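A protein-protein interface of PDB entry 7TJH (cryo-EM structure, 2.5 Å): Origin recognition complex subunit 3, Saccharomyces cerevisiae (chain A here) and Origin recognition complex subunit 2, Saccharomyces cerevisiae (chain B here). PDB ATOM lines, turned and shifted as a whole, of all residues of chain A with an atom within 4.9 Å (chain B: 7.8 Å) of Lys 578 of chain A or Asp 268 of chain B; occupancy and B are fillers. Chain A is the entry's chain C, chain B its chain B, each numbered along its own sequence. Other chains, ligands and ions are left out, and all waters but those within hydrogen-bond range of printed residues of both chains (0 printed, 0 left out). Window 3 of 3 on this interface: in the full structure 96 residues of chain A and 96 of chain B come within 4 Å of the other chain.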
ATOM      1  N   TYR A 541      -0.468   2.751  -2.859  1.00  0.00           N
ATOM      2  CA  TYR A 541      -1.502   2.950  -3.867  1.00  0.00           C
ATOM      3  C   TYR A 541      -2.188   4.305  -3.720  1.00  0.00           C
ATOM      4  O   TYR A 541      -2.545   4.919  -4.732  1.00  0.00           O
ATOM      5  CB  TYR A 541      -2.505   1.796  -3.787  1.00  0.00           C
ATOM      6  CG  TYR A 541      -3.902   2.093  -4.283  1.00  0.00           C
ATOM      7  CD1 TYR A 541      -4.161   2.297  -5.636  1.00  0.00           C
ATOM      8  CD2 TYR A 541      -4.969   2.149  -3.395  1.00  0.00           C
ATOM      9  CE1 TYR A 541      -5.444   2.572  -6.082  1.00  0.00           C
ATOM     10  CE2 TYR A 541      -6.251   2.413  -3.832  1.00  0.00           C
ATOM     11  CZ  TYR A 541      -6.482   2.623  -5.174  1.00  0.00           C
ATOM     12  OH  TYR A 541      -7.759   2.887  -5.604  1.00  0.00           O
ATOM     13  N   LEU A 569     -18.747   1.349 -16.641  1.00  0.00           N
ATOM     14  CA  LEU A 569     -17.849   1.456 -15.495  1.00  0.00           C
ATOM     15  C   LEU A 569     -17.456   2.905 -15.230  1.00  0.00           C
ATOM     16  O   LEU A 569     -17.287   3.296 -14.071  1.00  0.00           O
ATOM     17  CB  LEU A 569     -16.614   0.579 -15.716  1.00  0.00           C
ATOM     18  CG  LEU A 569     -15.490   0.592 -14.676  1.00  0.00           C
ATOM     19  CD1 LEU A 569     -16.023   0.258 -13.293  1.00  0.00           C
ATOM     20  CD2 LEU A 569     -14.412  -0.390 -15.070  1.00  0.00           C
ATOM     21  N   ASP A 574     -17.314   5.313  -8.286  1.00  0.00           N
ATOM     22  CA  ASP A 574     -16.040   4.791  -7.809  1.00  0.00           C
ATOM     23  C   ASP A 574     -15.153   4.315  -8.956  1.00  0.00           C
ATOM     24  O   ASP A 574     -14.420   3.332  -8.809  1.00  0.00           O
ATOM     25  CB  ASP A 574     -16.277   3.661  -6.809  1.00  0.00           C
ATOM     26  CG  ASP A 574     -15.193   3.579  -5.752  1.00  0.00           C
ATOM     27  OD1 ASP A 574     -15.200   4.421  -4.829  1.00  0.00           O
ATOM     28  OD2 ASP A 574     -14.336   2.675  -5.842  1.00  0.00           O
ATOM     29  N   ALA A 575     -15.219   4.995 -10.103  1.00  0.00           N
ATOM     30  CA  ALA A 575     -14.516   4.531 -11.295  1.00  0.00           C
ATOM     31  C   ALA A 575     -13.017   4.777 -11.199  1.00  0.00           C
ATOM     32  O   ALA A 575     -12.218   3.903 -11.563  1.00  0.00           O
ATOM     33  CB  ALA A 575     -15.085   5.219 -12.534  1.00  0.00           C
ATOM     34  N   PHE A 576     -12.621   5.959 -10.719  1.00  0.00           N
ATOM     35  CA  PHE A 576     -11.210   6.335 -10.707  1.00  0.00           C
ATOM     36  C   PHE A 576     -10.406   5.502  -9.719  1.00  0.00           C
ATOM     37  O   PHE A 576      -9.245   5.174  -9.990  1.00  0.00           O
ATOM     38  CB  PHE A 576     -11.064   7.828 -10.416  1.00  0.00           C
ATOM     39  CG  PHE A 576      -9.651   8.326 -10.527  1.00  0.00           C
ATOM     40  CD1 PHE A 576      -9.120   8.680 -11.754  1.00  0.00           C
ATOM     41  CD2 PHE A 576      -8.869   8.484  -9.388  1.00  0.00           C
ATOM     42  CE1 PHE A 576      -7.812   9.131 -11.850  1.00  0.00           C
ATOM     43  CE2 PHE A 576      -7.574   8.945  -9.476  1.00  0.00           C
ATOM     44  CZ  PHE A 576      -7.047   9.275 -10.706  1.00  0.00           C
ATOM     45  N   ASP A 577     -11.002   5.148  -8.577  1.00  0.00           N
ATOM     46  CA  ASP A 577     -10.326   4.272  -7.624  1.00  0.00           C
ATOM     47  C   ASP A 577     -10.095   2.887  -8.216  1.00  0.00           C
ATOM     48  O   ASP A 577      -9.022   2.299  -8.036  1.00  0.00           O
ATOM     49  CB  ASP A 577     -11.136   4.175  -6.333  1.00  0.00           C
ATOM     50  CG  ASP A 577     -11.525   5.534  -5.782  1.00  0.00           C
ATOM     51  OD1 ASP A 577     -10.837   6.527  -6.099  1.00  0.00           O
ATOM     52  OD2 ASP A 577     -12.516   5.608  -5.028  1.00  0.00           O
ATOM     53  N   LYS A 578     -11.080   2.368  -8.956  1.00  0.00           N
ATOM     54  CA  LYS A 578     -10.937   1.064  -9.596  1.00  0.00           C
ATOM     55  C   LYS A 578      -9.888   1.092 -10.702  1.00  0.00           C
ATOM     56  O   LYS A 578      -9.082   0.162 -10.815  1.00  0.00           O
ATOM     57  CB  LYS A 578     -12.284   0.603 -10.152  1.00  0.00           C
ATOM     58  CG  LYS A 578     -13.282   0.165  -9.095  1.00  0.00           C
ATOM     59  CD  LYS A 578     -14.548  -0.387  -9.732  1.00  0.00           C
ATOM     60  CE  LYS A 578     -15.535  -0.866  -8.681  1.00  0.00           C
ATOM     61  NZ  LYS A 578     -16.788  -1.396  -9.288  1.00  0.00           N
ATOM     62  N   VAL A 579      -9.879   2.154 -11.517  1.00  0.00           N
ATOM     63  CA  VAL A 579      -8.887   2.287 -12.586  1.00  0.00           C
ATOM     64  C   VAL A 579      -7.483   2.419 -11.999  1.00  0.00           C
ATOM     65  O   VAL A 579      -6.527   1.788 -12.480  1.00  0.00           O
ATOM     66  CB  VAL A 579      -9.248   3.478 -13.498  1.00  0.00           C
ATOM     67  CG1 VAL A 579      -8.106   3.831 -14.438  1.00  0.00           C
ATOM     68  CG2 VAL A 579     -10.505   3.172 -14.296  1.00  0.00           C
ATOM     69  N   ALA A 580      -7.352   3.206 -10.925  1.00  0.00           N
ATOM     70  CA  ALA A 580      -6.074   3.360 -10.240  1.00  0.00           C
ATOM     71  C   ALA A 580      -5.603   2.048  -9.626  1.00  0.00           C
ATOM     72  O   ALA A 580      -4.413   1.731  -9.684  1.00  0.00           O
ATOM     73  CB  ALA A 580      -6.187   4.447  -9.170  1.00  0.00           C
ATOM     74  N   LEU A 581      -6.524   1.253  -9.073  1.00  0.00           N
ATOM     75  CA  LEU A 581      -6.141  -0.031  -8.488  1.00  0.00           C
ATOM     76  C   LEU A 581      -5.725  -1.039  -9.553  1.00  0.00           C
ATOM     77  O   LEU A 581      -4.798  -1.826  -9.336  1.00  0.00           O
ATOM     78  CB  LEU A 581      -7.287  -0.588  -7.648  1.00  0.00           C
ATOM     79  CG  LEU A 581      -6.907  -1.752  -6.733  1.00  0.00           C
ATOM     80  CD1 LEU A 581      -6.328  -1.246  -5.418  1.00  0.00           C
ATOM     81  CD2 LEU A 581      -8.107  -2.650  -6.496  1.00  0.00           C
ATOM     82  N   ILE A 582      -6.394  -1.023 -10.707  1.00  0.00           N
ATOM     83  CA  ILE A 582      -6.052  -1.922 -11.809  1.00  0.00           C
ATOM     84  C   ILE A 582      -4.667  -1.590 -12.360  1.00  0.00           C
ATOM     85  O   ILE A 582      -3.803  -2.472 -12.514  1.00  0.00           O
ATOM     86  CB  ILE A 582      -7.144  -1.822 -12.890  1.00  0.00           C
ATOM     87  CG1 ILE A 582      -8.408  -2.540 -12.419  1.00  0.00           C
ATOM     88  CG2 ILE A 582      -6.665  -2.388 -14.217  1.00  0.00           C
ATOM     89  CD1 ILE A 582      -9.584  -2.323 -13.317  1.00  0.00           C
ATOM     90  N   MET B 263      -5.790  -4.223   2.316  1.00  0.00           N
ATOM     91  CA  MET B 263      -6.676  -4.175   1.160  1.00  0.00           C
ATOM     92  C   MET B 263      -8.153  -4.160   1.531  1.00  0.00           C
ATOM     93  O   MET B 263      -8.994  -4.057   0.631  1.00  0.00           O
ATOM     94  CB  MET B 263      -6.387  -5.363   0.240  1.00  0.00           C
ATOM     95  CG  MET B 263      -5.976  -4.986  -1.179  1.00  0.00           C
ATOM     96  SD  MET B 263      -4.891  -3.548  -1.303  1.00  0.00           S
ATOM     97  CE  MET B 263      -3.380  -4.154  -0.577  1.00  0.00           C
ATOM     98  N   SER B 264      -8.490  -4.281   2.818  1.00  0.00           N
ATOM     99  CA  SER B 264      -9.890  -4.216   3.227  1.00  0.00           C
ATOM    100  C   SER B 264     -10.467  -2.815   3.054  1.00  0.00           C
ATOM    101  O   SER B 264     -11.678  -2.666   2.857  1.00  0.00           O
ATOM    102  CB  SER B 264     -10.038  -4.674   4.676  1.00  0.00           C
ATOM    103  OG  SER B 264      -9.267  -3.864   5.546  1.00  0.00           O
ATOM    104  N   MET B 265      -9.628  -1.783   3.120  1.00  0.00           N
ATOM    105  CA  MET B 265     -10.049  -0.430   2.785  1.00  0.00           C
ATOM    106  C   MET B 265      -9.809  -0.078   1.321  1.00  0.00           C
ATOM    107  O   MET B 265      -9.991   1.081   0.940  1.00  0.00           O
ATOM    108  CB  MET B 265      -9.368   0.596   3.702  1.00  0.00           C
ATOM    109  CG  MET B 265      -7.882   0.409   3.908  1.00  0.00           C
ATOM    110  SD  MET B 265      -7.451   0.607   5.652  1.00  0.00           S
ATOM    111  CE  MET B 265      -7.639  -1.060   6.269  1.00  0.00           C
ATOM    112  N   ALA B 266      -9.414  -1.063   0.485  1.00  0.00           N
ATOM    113  CA  ALA B 266      -9.258  -0.857  -0.945  1.00  0.00           C
ATOM    114  C   ALA B 266     -10.512  -1.304  -1.693  1.00  0.00           C
ATOM    115  O   ALA B 266     -11.233  -2.189  -1.221  1.00  0.00           O
ATOM    116  CB  ALA B 266      -8.040  -1.625  -1.469  1.00  0.00           C
ATOM    117  N   PRO B 267     -10.818  -0.685  -2.837  1.00  0.00           N
ATOM    118  CA  PRO B 267     -11.985  -1.112  -3.622  1.00  0.00           C
ATOM    119  C   PRO B 267     -11.838  -2.523  -4.173  1.00  0.00           C
ATOM    120  O   PRO B 267     -10.739  -2.993  -4.472  1.00  0.00           O
ATOM    121  CB  PRO B 267     -12.043  -0.089  -4.761  1.00  0.00           C
ATOM    122  CG  PRO B 267     -11.341   1.101  -4.249  1.00  0.00           C
ATOM    123  CD  PRO B 267     -10.299   0.620  -3.289  1.00  0.00           C
ATOM    124  N   ASP B 268     -12.974  -3.202  -4.296  1.00  0.00           N
ATOM    125  CA  ASP B 268     -13.014  -4.549  -4.846  1.00  0.00           C
ATOM    126  C   ASP B 268     -13.288  -4.480  -6.342  1.00  0.00           C
ATOM    127  O   ASP B 268     -14.194  -3.766  -6.782  1.00  0.00           O
ATOM    128  CB  ASP B 268     -14.083  -5.388  -4.146  1.00  0.00           C
ATOM    129  CG  ASP B 268     -13.702  -5.748  -2.725  1.00  0.00           C
ATOM    130  OD1 ASP B 268     -12.491  -5.836  -2.436  1.00  0.00           O
ATOM    131  OD2 ASP B 268     -14.615  -5.943  -1.895  1.00  0.00           O
ATOM    132  N   VAL B 269     -12.497  -5.214  -7.119  1.00  0.00           N
ATOM    133  CA  VAL B 269     -12.656  -5.279  -8.564  1.00  0.00           C
ATOM    134  C   VAL B 269     -12.820  -6.735  -8.974  1.00  0.00           C
ATOM    135  O   VAL B 269     -12.333  -7.650  -8.302  1.00  0.00           O
ATOM    136  CB  VAL B 269     -11.469  -4.630  -9.312  1.00  0.00           C
ATOM    137  CG1 VAL B 269     -11.494  -3.122  -9.140  1.00  0.00           C
ATOM    138  CG2 VAL B 269     -10.148  -5.197  -8.817  1.00  0.00           C
ATOM    139  N   THR B 270     -13.529  -6.947 -10.078  1.00  0.00           N
ATOM    140  CA  THR B 270     -13.710  -8.284 -10.614  1.00  0.00           C
ATOM    141  C   THR B 270     -12.627  -8.576 -11.648  1.00  0.00           C
ATOM    142  O   THR B 270     -11.815  -7.716 -11.997  1.00  0.00           O
ATOM    143  CB  THR B 270     -15.107  -8.444 -11.215  1.00  0.00           C
ATOM    144  OG1 THR B 270     -15.288  -7.502 -12.279  1.00  0.00           O
ATOM    145  CG2 THR B 270     -16.171  -8.213 -10.153  1.00  0.00           C
ATOM    146  N   GLU B 273     -13.670  -6.638 -15.316  1.00  0.00           N
ATOM    147  CA  GLU B 273     -13.392  -5.208 -15.423  1.00  0.00           C
ATOM    148  C   GLU B 273     -11.896  -4.931 -15.359  1.00  0.00           C
ATOM    149  O   GLU B 273     -11.418  -3.976 -15.989  1.00  0.00           O
ATOM    150  CB  GLU B 273     -14.151  -4.422 -14.347  1.00  0.00           C
ATOM    151  CG  GLU B 273     -13.722  -4.660 -12.906  1.00  0.00           C
ATOM    152  CD  GLU B 273     -14.603  -3.929 -11.913  1.00  0.00           C
ATOM    153  OE1 GLU B 273     -14.946  -2.757 -12.173  1.00  0.00           O
ATOM    154  OE2 GLU B 273     -14.961  -4.529 -10.879  1.00  0.00           O
ATOM    155  N   PHE B 274     -11.148  -5.780 -14.641  1.00  0.00           N
ATOM    156  CA  PHE B 274      -9.693  -5.705 -14.652  1.00  0.00           C
ATOM    157  C   PHE B 274      -9.152  -5.949 -16.051  1.00  0.00           C
ATOM    158  O   PHE B 274      -8.321  -5.179 -16.547  1.00  0.00           O
ATOM    159  CB  PHE B 274      -9.101  -6.707 -13.658  1.00  0.00           C
ATOM    160  CG  PHE B 274      -7.599  -6.793 -13.705  1.00  0.00           C
ATOM    161  CD1 PHE B 274      -6.829  -5.811 -13.111  1.00  0.00           C
ATOM    162  CD2 PHE B 274      -6.962  -7.862 -14.319  1.00  0.00           C
ATOM    163  CE1 PHE B 274      -5.448  -5.873 -13.147  1.00  0.00           C
ATOM    164  CE2 PHE B 274      -5.581  -7.936 -14.357  1.00  0.00           C
ATOM    165  CZ  PHE B 274      -4.824  -6.938 -13.772  1.00  0.00           C
ATOM    166  N   VAL B 277     -10.304  -2.810 -18.487  1.00  0.00           N
ATOM    167  CA  VAL B 277      -9.470  -1.624 -18.302  1.00  0.00           C
ATOM    168  C   VAL B 277      -8.029  -1.915 -18.706  1.00  0.00           C
ATOM    169  O   VAL B 277      -7.350  -1.045 -19.277  1.00  0.00           O
ATOM    170  CB  VAL B 277      -9.582  -1.124 -16.845  1.00  0.00           C
ATOM    171  CG1 VAL B 277      -8.656   0.059 -16.567  1.00  0.00           C
ATOM    172  CG2 VAL B 277     -11.009  -0.732 -16.542  1.00  0.00           C
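Of the 11 printed residues of chain B, 6 touch a printed residue of chain A. Printed residues of chain B that touch a printed residue of chain A: Pro 267, Asp 268, Val 269, Glu 273, Phe 274 and Val 277. Printed residues of chain A that touch a printed residue of chain B: Leu 569, Asp 574, Asp 577, Lys 578, Leu 581 and Ile 582. Along chain A the printed residues that touch a printed residue of chain B span positions 569 to 582.
The side-chain carboxylate of Glu 273 of chain B is in hydrogen-bond range of the backbone NH of Thr 270 of chain B, 2.9 Å away. The backbone carbonyl oxygen (O) of Asp 577 of chain A sits at hydrogen-bond distance from the side-chain hydroxyl (OH) of Tyr 541 of chain A, 2.8 Å away.
Printed residues of chain B within 4 Å of Asp 574 of chain A: Pro 267. Phe 576 of chain A touches none of the printed residues of chain B. Of the printed residues of chain B, Asp 577 of chain A touches Pro 267. Of the printed residues of chain B, Leu 581 of chain A touches Pro 267 (3.3 Å). Asp 268 of chain B touches just one residue of chain A: Lys 578. Of the printed residues of chain A, Val 277 of chain B touches Leu 569 and Ile 582. The nearest printed residue of chain B that does not touch Leu 569 of chain A is Phe 274 of chain B (6.3 Å).
NZ of Lys 578 of chain A lies within salt-bridge range of OE1 of Glu 273 of chain B (3.7 Å).
Leu 569 of chain A touches Glu 273 of chain B. Val 277 of chain B touches Leu 569 of chain A (CG2 to CD2, 3.7 Å). Pro 267 of chain B touches Asp 574 of chain A (CG to OD2, 3.7 Å). Pro 267 of chain B touches Asp 577 of chain A. Lys 578 of chain A touches Asp 268 of chain B (CE to O, 3.7 Å). Val 269 of chain B touches Lys 578 of chain A. CD2 of Leu 581 of chain A touches O of Pro 267 of chain B, 3.3 Å away. Ile 582 of chain A touches Glu 273 of chain B. CG2 of Ile 582 of chain A touches CD1 of Phe 274 of chain B, at 3.6 Å. CB of Val 277 of chain B touches CD1 of Ile 582 of chain A (3.7 Å).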
